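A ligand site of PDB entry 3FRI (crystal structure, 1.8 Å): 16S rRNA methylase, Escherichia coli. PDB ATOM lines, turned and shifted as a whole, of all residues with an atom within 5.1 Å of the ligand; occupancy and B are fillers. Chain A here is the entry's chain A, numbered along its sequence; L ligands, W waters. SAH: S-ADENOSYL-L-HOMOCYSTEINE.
Water W4 lies within hydrogen-bond range of O3' of the ligand (2.6 Å), O of Cys 55 (3.0 Å) and NE2 of His 83 (3.0 Å).
Water W5 lies within hydrogen-bond range of OXT of the ligand, N of Leu 116 and ND1 of His 83.
Water W3 bridges a nitrogen (N7) of the ligand (2.8 Å) and the guanidinium group (NH2) of Arg 28 (3.0 Å).
Water W1 lies within hydrogen-bond range of OD1 of Asp 111, N of the ligand and ND2 of Asn 117.
Water W2 lies within hydrogen-bond range of O of Ile 112 (2.6 Å), OD1 of Asp 111 (2.9 Å), N of Phe 175 (3.0 Å) and N of the ligand (3.1 Å).
NH2 of Arg 28 touches N6 of the ligand, at 3.7 Å.
Ile 54 touches the ligand.
CA of Cys 55 touches O2' of the ligand, 3.6 Å away.
CG2 of Thr 86 touches OXT of the ligand (3.7 Å).
Cys 114 touches the ligand (O to CA, 3.5 Å).
Gly 115 touches the ligand.
Ile 134 touches the ligand.
Gln 158 touches the ligand.
Leu 161 touches the ligand (CG to N6, 3.9 Å).
O of Lys 176 touches C5' of the ligand, at 3.6 Å.
CD1 of Leu 177 touches O4' of the ligand, at 3.7 Å.
CD1 of Leu 180 touches C5' of the ligand (3.9 Å).
CD2 of Leu 181 touches N6 of the ligand, 3.9 Å away.
N of Cys 114 sits at hydrogen-bond distance from O of Cys 132.
The guanidinium group of Arg 89 lies within salt-bridge range of the side-chain carboxylate of Glu 244, at 2.8 Å.
The backbone NH (N) of Ser 85 is in hydrogen-bond range of a ring nitrogen (ND1) of His 83, at 3.1 Å.
N of Ala 113 is in hydrogen-bond range of O of Cys 132 (2.8 Å).
The backbone NH of Gln 158 lies within hydrogen-bond range of the backbone carbonyl oxygen of Asp 133 (3.0 Å).
OD1 of Asp 159 sits at hydrogen-bond distance from N of Leu 161 (2.9 Å).
The side-chain hydroxyl (OG1) of Thr 86 sits at hydrogen-bond distance from the backbone carbonyl oxygen (O) of His 83 (3.0 Å).
The backbone NH of Cys 114 sits at hydrogen-bond distance from the side-chain carboxylate of Asp 133 (3.4 Å).
O of the ligand is in salt-bridge range of NH2 of Arg 89, at 2.7 Å.
An oxygen (OXT) of the ligand sits at hydrogen-bond distance from the side-chain hydroxyl (OG) of Ser 85 (2.8 Å).
The backbone carbonyl oxygen of Ala 113 sits at hydrogen-bond distance from a nitrogen (N) of the ligand (2.7 Å).
N of the ligand sits at hydrogen-bond distance from O of Phe 175 (2.9 Å).
N of Val 160 sits at hydrogen-bond distance from N1 of the ligand (3.1 Å).
A nitrogen (N6) of the ligand is in hydrogen-bond range of the side-chain carboxylate (OD1) of Asp 159 (2.8 Å).
OD1 of Asp 133 sits at hydrogen-bond distance from O2' of the ligand (2.7 Å).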
ATOM      1  N   ARG A  28     -30.158  30.772 -13.794  1.00  0.00           N
ATOM      2  CA  ARG A  28     -29.683  31.528 -12.638  1.00  0.00           C
ATOM      3  C   ARG A  28     -28.481  32.402 -12.996  1.00  0.00           C
ATOM      4  O   ARG A  28     -28.477  33.610 -12.756  1.00  0.00           O
ATOM      5  CB  ARG A  28     -29.309  30.579 -11.494  1.00  0.00           C
ATOM      6  CG  ARG A  28     -28.766  31.267 -10.252  1.00  0.00           C
ATOM      7  CD  ARG A  28     -28.758  30.337  -9.046  1.00  0.00           C
ATOM      8  NE  ARG A  28     -27.931  29.144  -9.241  1.00  0.00           N
ATOM      9  CZ  ARG A  28     -26.600  29.132  -9.202  1.00  0.00           C
ATOM     10  NH1 ARG A  28     -25.923  30.251  -8.977  1.00  0.00           N
ATOM     11  NH2 ARG A  28     -25.939  27.988  -9.389  1.00  0.00           N
ATOM     12  N   ILE A  54     -18.698  25.244 -12.721  1.00  0.00           N
ATOM     13  CA  ILE A  54     -19.842  25.155 -11.813  1.00  0.00           C
ATOM     14  C   ILE A  54     -20.060  23.742 -11.238  1.00  0.00           C
ATOM     15  O   ILE A  54     -20.651  23.590 -10.178  1.00  0.00           O
ATOM     16  CB  ILE A  54     -21.143  25.635 -12.523  1.00  0.00           C
ATOM     17  CG1 ILE A  54     -22.165  26.117 -11.485  1.00  0.00           C
ATOM     18  CG2 ILE A  54     -21.732  24.526 -13.373  1.00  0.00           C
ATOM     19  CD1 ILE A  54     -21.983  27.569 -11.081  1.00  0.00           C
ATOM     20  N   CYS A  55     -19.563  22.713 -11.937  1.00  0.00           N
ATOM     21  CA  CYS A  55     -19.734  21.332 -11.468  1.00  0.00           C
ATOM     22  C   CYS A  55     -18.482  20.654 -10.921  1.00  0.00           C
ATOM     23  O   CYS A  55     -18.573  19.587 -10.307  1.00  0.00           O
ATOM     24  CB  CYS A  55     -20.320  20.471 -12.591  1.00  0.00           C
ATOM     25  SG  CYS A  55     -22.016  20.866 -13.048  1.00  0.00           S
ATOM     26  N   HIS A  83     -14.502  10.499  -9.744  1.00  0.00           N
ATOM     27  CA  HIS A  83     -15.074  11.811  -9.429  1.00  0.00           C
ATOM     28  C   HIS A  83     -14.177  12.350  -8.325  1.00  0.00           C
ATOM     29  O   HIS A  83     -14.032  11.730  -7.272  1.00  0.00           O
ATOM     30  CB  HIS A  83     -16.522  11.723  -8.930  1.00  0.00           C
ATOM     31  CG  HIS A  83     -17.149  13.070  -8.711  1.00  0.00           C
ATOM     32  ND1 HIS A  83     -16.790  13.903  -7.682  1.00  0.00           N
ATOM     33  CD2 HIS A  83     -18.076  13.749  -9.436  1.00  0.00           C
ATOM     34  CE1 HIS A  83     -17.455  15.040  -7.782  1.00  0.00           C
ATOM     35  NE2 HIS A  83     -18.248  14.973  -8.834  1.00  0.00           N
ATOM     36  N   SER A  85     -14.261  14.488  -5.909  1.00  0.00           N
ATOM     37  CA  SER A  85     -14.685  14.574  -4.519  1.00  0.00           C
ATOM     38  C   SER A  85     -14.741  13.234  -3.790  1.00  0.00           C
ATOM     39  O   SER A  85     -14.359  13.149  -2.627  1.00  0.00           O
ATOM     40  CB  SER A  85     -16.040  15.266  -4.420  1.00  0.00           C
ATOM     41  OG  SER A  85     -16.358  15.489  -3.056  1.00  0.00           O
ATOM     42  N   THR A  86     -15.224  12.206  -4.465  1.00  0.00           N
ATOM     43  CA  THR A  86     -15.297  10.894  -3.848  1.00  0.00           C
ATOM     44  C   THR A  86     -13.941  10.206  -3.835  1.00  0.00           C
ATOM     45  O   THR A  86     -13.656   9.407  -2.945  1.00  0.00           O
ATOM     46  CB  THR A  86     -16.343   9.988  -4.545  1.00  0.00           C
ATOM     47  OG1 THR A  86     -16.278  10.163  -5.961  1.00  0.00           O
ATOM     48  CG2 THR A  86     -17.735  10.310  -4.050  1.00  0.00           C
ATOM     49  N   ARG A  89     -11.804  11.019  -0.877  1.00  0.00           N
ATOM     50  CA  ARG A  89     -12.416  10.494   0.339  1.00  0.00           C
ATOM     51  C   ARG A  89     -12.177   8.999   0.512  1.00  0.00           C
ATOM     52  O   ARG A  89     -12.380   8.430   1.588  1.00  0.00           O
ATOM     53  CB  ARG A  89     -13.936  10.771   0.300  1.00  0.00           C
ATOM     54  CG  ARG A  89     -14.707  10.294   1.513  1.00  0.00           C
ATOM     55  CD  ARG A  89     -16.193  10.672   1.416  1.00  0.00           C
ATOM     56  NE  ARG A  89     -16.392  12.120   1.384  1.00  0.00           N
ATOM     57  CZ  ARG A  89     -16.981  12.779   0.397  1.00  0.00           C
ATOM     58  NH1 ARG A  89     -17.444  12.126  -0.660  1.00  0.00           N
ATOM     59  NH2 ARG A  89     -17.096  14.099   0.464  1.00  0.00           N
ATOM     60  N   ASP A 111     -28.892  13.219   0.071  1.00  0.00           N
ATOM     61  CA  ASP A 111     -27.527  13.611  -0.269  1.00  0.00           C
ATOM     62  C   ASP A 111     -27.640  14.872  -1.129  1.00  0.00           C
ATOM     63  O   ASP A 111     -27.939  14.781  -2.321  1.00  0.00           O
ATOM     64  CB  ASP A 111     -26.855  12.470  -1.053  1.00  0.00           C
ATOM     65  CG  ASP A 111     -25.347  12.532  -0.997  1.00  0.00           C
ATOM     66  OD1 ASP A 111     -24.800  13.609  -0.669  1.00  0.00           O
ATOM     67  OD2 ASP A 111     -24.706  11.506  -1.315  1.00  0.00           O
ATOM     68  N   ILE A 112     -27.409  16.030  -0.520  1.00  0.00           N
ATOM     69  CA  ILE A 112     -27.523  17.335  -1.200  1.00  0.00           C
ATOM     70  C   ILE A 112     -26.248  17.689  -1.990  1.00  0.00           C
ATOM     71  O   ILE A 112     -25.175  17.817  -1.400  1.00  0.00           O
ATOM     72  CB  ILE A 112     -27.811  18.437  -0.151  1.00  0.00           C
ATOM     73  CG1 ILE A 112     -28.862  17.942   0.843  1.00  0.00           C
ATOM     74  CG2 ILE A 112     -28.302  19.711  -0.844  1.00  0.00           C
ATOM     75  CD1 ILE A 112     -30.162  17.470   0.224  1.00  0.00           C
ATOM     76  N   ALA A 113     -26.400  17.861  -3.301  1.00  0.00           N
ATOM     77  CA  ALA A 113     -25.272  18.133  -4.215  1.00  0.00           C
ATOM     78  C   ALA A 113     -24.448  16.850  -4.092  1.00  0.00           C
ATOM     79  O   ALA A 113     -23.251  16.856  -3.792  1.00  0.00           O
ATOM     80  CB  ALA A 113     -24.471  19.344  -3.727  1.00  0.00           C
ATOM     81  N   CYS A 114     -25.121  15.735  -4.349  1.00  0.00           N
ATOM     82  CA  CYS A 114     -24.556  14.403  -4.199  1.00  0.00           C
ATOM     83  C   CYS A 114     -23.326  13.943  -4.964  1.00  0.00           C
ATOM     84  O   CYS A 114     -22.600  13.084  -4.466  1.00  0.00           O
ATOM     85  CB  CYS A 114     -25.657  13.365  -4.388  1.00  0.00           C
ATOM     86  SG  CYS A 114     -26.274  13.225  -6.084  1.00  0.00           S
ATOM     87  N   GLY A 115     -23.074  14.491  -6.151  1.00  0.00           N
ATOM     88  CA  GLY A 115     -21.918  14.019  -6.920  1.00  0.00           C
ATOM     89  C   GLY A 115     -22.096  12.520  -7.052  1.00  0.00           C
ATOM     90  O   GLY A 115     -23.198  12.059  -7.333  1.00  0.00           O
ATOM     91  N   LEU A 116     -21.027  11.735  -6.857  1.00  0.00           N
ATOM     92  CA  LEU A 116     -21.150  10.277  -6.944  1.00  0.00           C
ATOM     93  C   LEU A 116     -21.173   9.583  -5.583  1.00  0.00           C
ATOM     94  O   LEU A 116     -21.179   8.358  -5.492  1.00  0.00           O
ATOM     95  CB  LEU A 116     -20.004   9.675  -7.779  1.00  0.00           C
ATOM     96  CG  LEU A 116     -20.024   9.950  -9.282  1.00  0.00           C
ATOM     97  CD1 LEU A 116     -18.931   9.111  -9.958  1.00  0.00           C
ATOM     98  CD2 LEU A 116     -21.385   9.590  -9.870  1.00  0.00           C
ATOM     99  N   ASN A 117     -21.221  10.377  -4.508  1.00  0.00           N
ATOM    100  CA  ASN A 117     -21.238   9.823  -3.163  1.00  0.00           C
ATOM    101  C   ASN A 117     -22.320   8.760  -2.902  1.00  0.00           C
ATOM    102  O   ASN A 117     -22.108   7.846  -2.099  1.00  0.00           O
ATOM    103  CB  ASN A 117     -21.364  10.935  -2.128  1.00  0.00           C
ATOM    104  CG  ASN A 117     -21.373  10.409  -0.705  1.00  0.00           C
ATOM    105  OD1 ASN A 117     -20.378   9.883  -0.225  1.00  0.00           O
ATOM    106  ND2 ASN A 117     -22.513  10.533  -0.035  1.00  0.00           N
ATOM    107  N   CYS A 132     -29.558  14.999  -5.021  1.00  0.00           N
ATOM    108  CA  CYS A 132     -29.788  16.008  -6.047  1.00  0.00           C
ATOM    109  C   CYS A 132     -28.485  16.694  -6.436  1.00  0.00           C
ATOM    110  O   CYS A 132     -27.587  16.863  -5.610  1.00  0.00           O
ATOM    111  CB  CYS A 132     -30.808  17.056  -5.572  1.00  0.00           C
ATOM    112  SG  CYS A 132     -30.252  18.152  -4.232  1.00  0.00           S
ATOM    113  N   ASP A 133     -28.376  17.047  -7.696  1.00  0.00           N
ATOM    114  CA  ASP A 133     -27.189  17.745  -8.166  1.00  0.00           C
ATOM    115  C   ASP A 133     -27.587  18.477  -9.445  1.00  0.00           C
ATOM    116  O   ASP A 133     -28.718  18.342  -9.899  1.00  0.00           O
ATOM    117  CB  ASP A 133     -26.034  16.763  -8.408  1.00  0.00           C
ATOM    118  CG  ASP A 133     -24.674  17.400  -8.188  1.00  0.00           C
ATOM    119  OD1 ASP A 133     -24.341  18.329  -8.950  1.00  0.00           O
ATOM    120  OD2 ASP A 133     -23.948  16.993  -7.256  1.00  0.00           O
ATOM    121  N   ILE A 134     -26.655  19.242 -10.014  1.00  0.00           N
ATOM    122  CA  ILE A 134     -26.951  20.013 -11.215  1.00  0.00           C
ATOM    123  C   ILE A 134     -26.404  19.447 -12.528  1.00  0.00           C
ATOM    124  O   ILE A 134     -26.460  20.099 -13.571  1.00  0.00           O
ATOM    125  CB  ILE A 134     -26.467  21.460 -11.058  1.00  0.00           C
ATOM    126  CG1 ILE A 134     -24.991  21.489 -10.653  1.00  0.00           C
ATOM    127  CG2 ILE A 134     -27.323  22.159 -10.004  1.00  0.00           C
ATOM    128  CD1 ILE A 134     -24.389  22.890 -10.596  1.00  0.00           C
ATOM    129  N   LEU A 138     -24.386  12.715 -13.564  1.00  0.00           N
ATOM    130  CA  LEU A 138     -24.239  12.032 -12.290  1.00  0.00           C
ATOM    131  C   LEU A 138     -25.380  11.051 -12.077  1.00  0.00           C
ATOM    132  O   LEU A 138     -25.167   9.915 -11.650  1.00  0.00           O
ATOM    133  CB  LEU A 138     -24.192  13.057 -11.147  1.00  0.00           C
ATOM    134  CG  LEU A 138     -23.042  14.058 -11.272  1.00  0.00           C
ATOM    135  CD1 LEU A 138     -23.233  15.211 -10.289  1.00  0.00           C
ATOM    136  CD2 LEU A 138     -21.727  13.353 -11.033  1.00  0.00           C
ATOM    137  N   GLN A 158     -31.587  19.193  -9.725  1.00  0.00           N
ATOM    138  CA  GLN A 158     -32.095  20.366  -9.018  1.00  0.00           C
ATOM    139  C   GLN A 158     -31.004  21.288  -8.476  1.00  0.00           C
ATOM    140  O   GLN A 158     -30.045  20.835  -7.853  1.00  0.00           O
ATOM    141  CB  GLN A 158     -32.980  19.884  -7.864  1.00  0.00           C
ATOM    142  CG  GLN A 158     -33.688  20.970  -7.066  1.00  0.00           C
ATOM    143  CD  GLN A 158     -34.591  20.389  -5.990  1.00  0.00           C
ATOM    144  OE1 GLN A 158     -35.086  19.271  -6.119  1.00  0.00           O
ATOM    145  NE2 GLN A 158     -34.808  21.150  -4.919  1.00  0.00           N
ATOM    146  N   ASP A 159     -31.161  22.592  -8.727  1.00  0.00           N
ATOM    147  CA  ASP A 159     -30.232  23.607  -8.234  1.00  0.00           C
ATOM    148  C   ASP A 159     -30.843  24.060  -6.907  1.00  0.00           C
ATOM    149  O   ASP A 159     -31.945  24.613  -6.885  1.00  0.00           O
ATOM    150  CB  ASP A 159     -30.164  24.781  -9.215  1.00  0.00           C
ATOM    151  CG  ASP A 159     -29.089  25.772  -8.861  1.00  0.00           C
ATOM    152  OD1 ASP A 159     -29.023  26.220  -7.691  1.00  0.00           O
ATOM    153  OD2 ASP A 159     -28.298  26.124  -9.767  1.00  0.00           O
ATOM    154  N   VAL A 160     -30.142  23.840  -5.805  1.00  0.00           N
ATOM    155  CA  VAL A 160     -30.697  24.213  -4.501  1.00  0.00           C
ATOM    156  C   VAL A 160     -30.827  25.711  -4.254  1.00  0.00           C
ATOM    157  O   VAL A 160     -31.494  26.122  -3.301  1.00  0.00           O
ATOM    158  CB  VAL A 160     -29.899  23.574  -3.343  1.00  0.00           C
ATOM    159  CG1 VAL A 160     -29.999  22.052  -3.427  1.00  0.00           C
ATOM    160  CG2 VAL A 160     -28.452  24.023  -3.397  1.00  0.00           C
ATOM    161  N   LEU A 161     -30.194  26.526  -5.085  1.00  0.00           N
ATOM    162  CA  LEU A 161     -30.305  27.970  -4.919  1.00  0.00           C
ATOM    163  C   LEU A 161     -31.598  28.445  -5.590  1.00  0.00           C
ATOM    164  O   LEU A 161     -32.044  29.575  -5.394  1.00  0.00           O
ATOM    165  CB  LEU A 161     -29.099  28.681  -5.517  1.00  0.00           C
ATOM    166  CG  LEU A 161     -27.750  28.436  -4.831  1.00  0.00           C
ATOM    167  CD1 LEU A 161     -26.637  29.146  -5.595  1.00  0.00           C
ATOM    168  CD2 LEU A 161     -27.812  28.933  -3.395  1.00  0.00           C
ATOM    169  N   PHE A 175     -21.989  17.575   2.000  1.00  0.00           N
ATOM    170  CA  PHE A 175     -20.538  17.468   1.881  1.00  0.00           C
ATOM    171  C   PHE A 175     -19.914  18.378   0.826  1.00  0.00           C
ATOM    172  O   PHE A 175     -20.276  18.328  -0.347  1.00  0.00           O
ATOM    173  CB  PHE A 175     -20.123  16.027   1.530  1.00  0.00           C
ATOM    174  CG  PHE A 175     -20.430  15.003   2.604  1.00  0.00           C
ATOM    175  CD1 PHE A 175     -20.212  13.647   2.345  1.00  0.00           C
ATOM    176  CD2 PHE A 175     -20.926  15.372   3.845  1.00  0.00           C
ATOM    177  CE1 PHE A 175     -20.478  12.677   3.324  1.00  0.00           C
ATOM    178  CE2 PHE A 175     -21.201  14.403   4.826  1.00  0.00           C
ATOM    179  CZ  PHE A 175     -20.972  13.065   4.563  1.00  0.00           C
ATOM    180  N   LYS A 176     -18.959  19.210   1.262  1.00  0.00           N
ATOM    181  CA  LYS A 176     -18.236  20.108   0.362  1.00  0.00           C
ATOM    182  C   LYS A 176     -19.139  20.966  -0.531  1.00  0.00           C
ATOM    183  O   LYS A 176     -18.871  21.126  -1.731  1.00  0.00           O
ATOM    184  CB  LYS A 176     -17.282  19.279  -0.513  1.00  0.00           C
ATOM    185  CG  LYS A 176     -16.338  18.360   0.256  1.00  0.00           C
ATOM    186  CD  LYS A 176     -15.589  17.422  -0.699  1.00  0.00           C
ATOM    187  CE  LYS A 176     -14.678  16.452   0.040  1.00  0.00           C
ATOM    188  NZ  LYS A 176     -14.087  15.425  -0.873  1.00  0.00           N
ATOM    189  N   LEU A 177     -20.195  21.526   0.055  1.00  0.00           N
ATOM    190  CA  LEU A 177     -21.130  22.344  -0.704  1.00  0.00           C
ATOM    191  C   LEU A 177     -21.329  23.773  -0.180  1.00  0.00           C
ATOM    192  O   LEU A 177     -21.411  24.715  -0.972  1.00  0.00           O
ATOM    193  CB  LEU A 177     -22.497  21.658  -0.764  1.00  0.00           C
ATOM    194  CG  LEU A 177     -23.626  22.447  -1.439  1.00  0.00           C
ATOM    195  CD1 LEU A 177     -23.328  22.618  -2.924  1.00  0.00           C
ATOM    196  CD2 LEU A 177     -24.944  21.697  -1.245  1.00  0.00           C
ATOM    197  N   LEU A 180     -19.125  26.721  -1.681  1.00  0.00           N
ATOM    198  CA  LEU A 180     -19.494  27.103  -3.042  1.00  0.00           C
ATOM    199  C   LEU A 180     -20.772  27.923  -3.065  1.00  0.00           C
ATOM    200  O   LEU A 180     -20.848  28.937  -3.763  1.00  0.00           O
ATOM    201  CB  LEU A 180     -19.694  25.866  -3.916  1.00  0.00           C
ATOM    202  CG  LEU A 180     -18.540  24.880  -4.107  1.00  0.00           C
ATOM    203  CD1 LEU A 180     -19.041  23.694  -4.925  1.00  0.00           C
ATOM    204  CD2 LEU A 180     -17.374  25.573  -4.797  1.00  0.00           C
ATOM    205  N   LEU A 181     -21.772  27.472  -2.321  1.00  0.00           N
ATOM    206  CA  LEU A 181     -23.063  28.162  -2.266  1.00  0.00           C
ATOM    207  C   LEU A 181     -22.949  29.571  -1.701  1.00  0.00           C
ATOM    208  O   LEU A 181     -23.502  30.514  -2.263  1.00  0.00           O
ATOM    209  CB  LEU A 181     -24.066  27.390  -1.416  1.00  0.00           C
ATOM    210  CG  LEU A 181     -24.582  26.042  -1.926  1.00  0.00           C
ATOM    211  CD1 LEU A 181     -25.532  25.462  -0.881  1.00  0.00           C
ATOM    212  CD2 LEU A 181     -25.292  26.214  -3.257  1.00  0.00           C
ATOM    213  N   GLU A 244     -11.499  16.184   5.117  1.00  0.00           N
ATOM    214  CA  GLU A 244     -12.714  16.889   5.514  1.00  0.00           C
ATOM    215  C   GLU A 244     -12.899  17.163   7.000  1.00  0.00           C
ATOM    216  O   GLU A 244     -12.554  16.342   7.849  1.00  0.00           O
ATOM    217  CB  GLU A 244     -13.954  16.116   5.048  1.00  0.00           C
ATOM    218  CG  GLU A 244     -14.027  15.812   3.577  1.00  0.00           C
ATOM    219  CD  GLU A 244     -15.190  14.895   3.244  1.00  0.00           C
ATOM    220  OE1 GLU A 244     -16.314  15.397   3.019  1.00  0.00           O
ATOM    221  OE2 GLU A 244     -14.983  13.661   3.221  1.00  0.00           O
HETATM  222  N   SAH L   1     -21.257  16.136  -2.058  1.00  0.00           N
HETATM  223  CA  SAH L   1     -20.419  15.410  -3.023  1.00  0.00           C
HETATM  224  CB  SAH L   1     -19.908  16.343  -4.149  1.00  0.00           C
HETATM  225  CG  SAH L   1     -19.134  17.547  -3.584  1.00  0.00           C
HETATM  226  SD  SAH L   1     -18.511  18.579  -4.949  1.00  0.00           S
HETATM  227  C   SAH L   1     -19.232  14.789  -2.325  1.00  0.00           C
HETATM  228  O   SAH L   1     -18.838  15.246  -1.274  1.00  0.00           O
HETATM  229  OXT SAH L   1     -18.597  13.752  -2.888  1.00  0.00           O
HETATM  230  C5' SAH L   1     -19.760  19.898  -5.010  1.00  0.00           C
HETATM  231  C4' SAH L   1     -21.031  19.428  -5.748  1.00  0.00           C
HETATM  232  O4' SAH L   1     -22.023  20.445  -5.645  1.00  0.00           O
HETATM  233  C3' SAH L   1     -20.784  19.175  -7.249  1.00  0.00           C
HETATM  234  O3' SAH L   1     -21.196  17.837  -7.597  1.00  0.00           O
HETATM  235  C2' SAH L   1     -21.630  20.265  -7.952  1.00  0.00           C
HETATM  236  O2' SAH L   1     -22.143  19.834  -9.218  1.00  0.00           O
HETATM  237  C1' SAH L   1     -22.733  20.514  -6.903  1.00  0.00           C
HETATM  238  N9  SAH L   1     -23.367  21.843  -6.978  1.00  0.00           N
HETATM  239  C8  SAH L   1     -22.768  23.051  -7.239  1.00  0.00           C
HETATM  240  N7  SAH L   1     -23.668  24.000  -7.198  1.00  0.00           N
HETATM  241  C5  SAH L   1     -24.872  23.459  -6.927  1.00  0.00           C
HETATM  242  C6  SAH L   1     -26.189  23.963  -6.764  1.00  0.00           C
HETATM  243  N6  SAH L   1     -26.445  25.326  -6.878  1.00  0.00           N
HETATM  244  N1  SAH L   1     -27.200  23.097  -6.487  1.00  0.00           N
HETATM  245  C2  SAH L   1     -26.976  21.780  -6.361  1.00  0.00           C
HETATM  246  N3  SAH L   1     -25.748  21.269  -6.505  1.00  0.00           N
HETATM  247  C4  SAH L   1     -24.696  22.068  -6.784  1.00  0.00           C
HETATM  248  O   HOH W   1     -22.012  13.688  -0.699  1.00  0.00           O
HETATM  249  O   HOH W   2     -23.611  16.187  -0.097  1.00  0.00           O
HETATM  250  O   HOH W   3     -23.573  26.724  -8.011  1.00  0.00           O
HETATM  251  O   HOH W   4     -20.116  17.068  -9.858  1.00  0.00           O
HETATM  252  O   HOH W   5     -18.942  13.170  -5.495  1.00  0.00           O
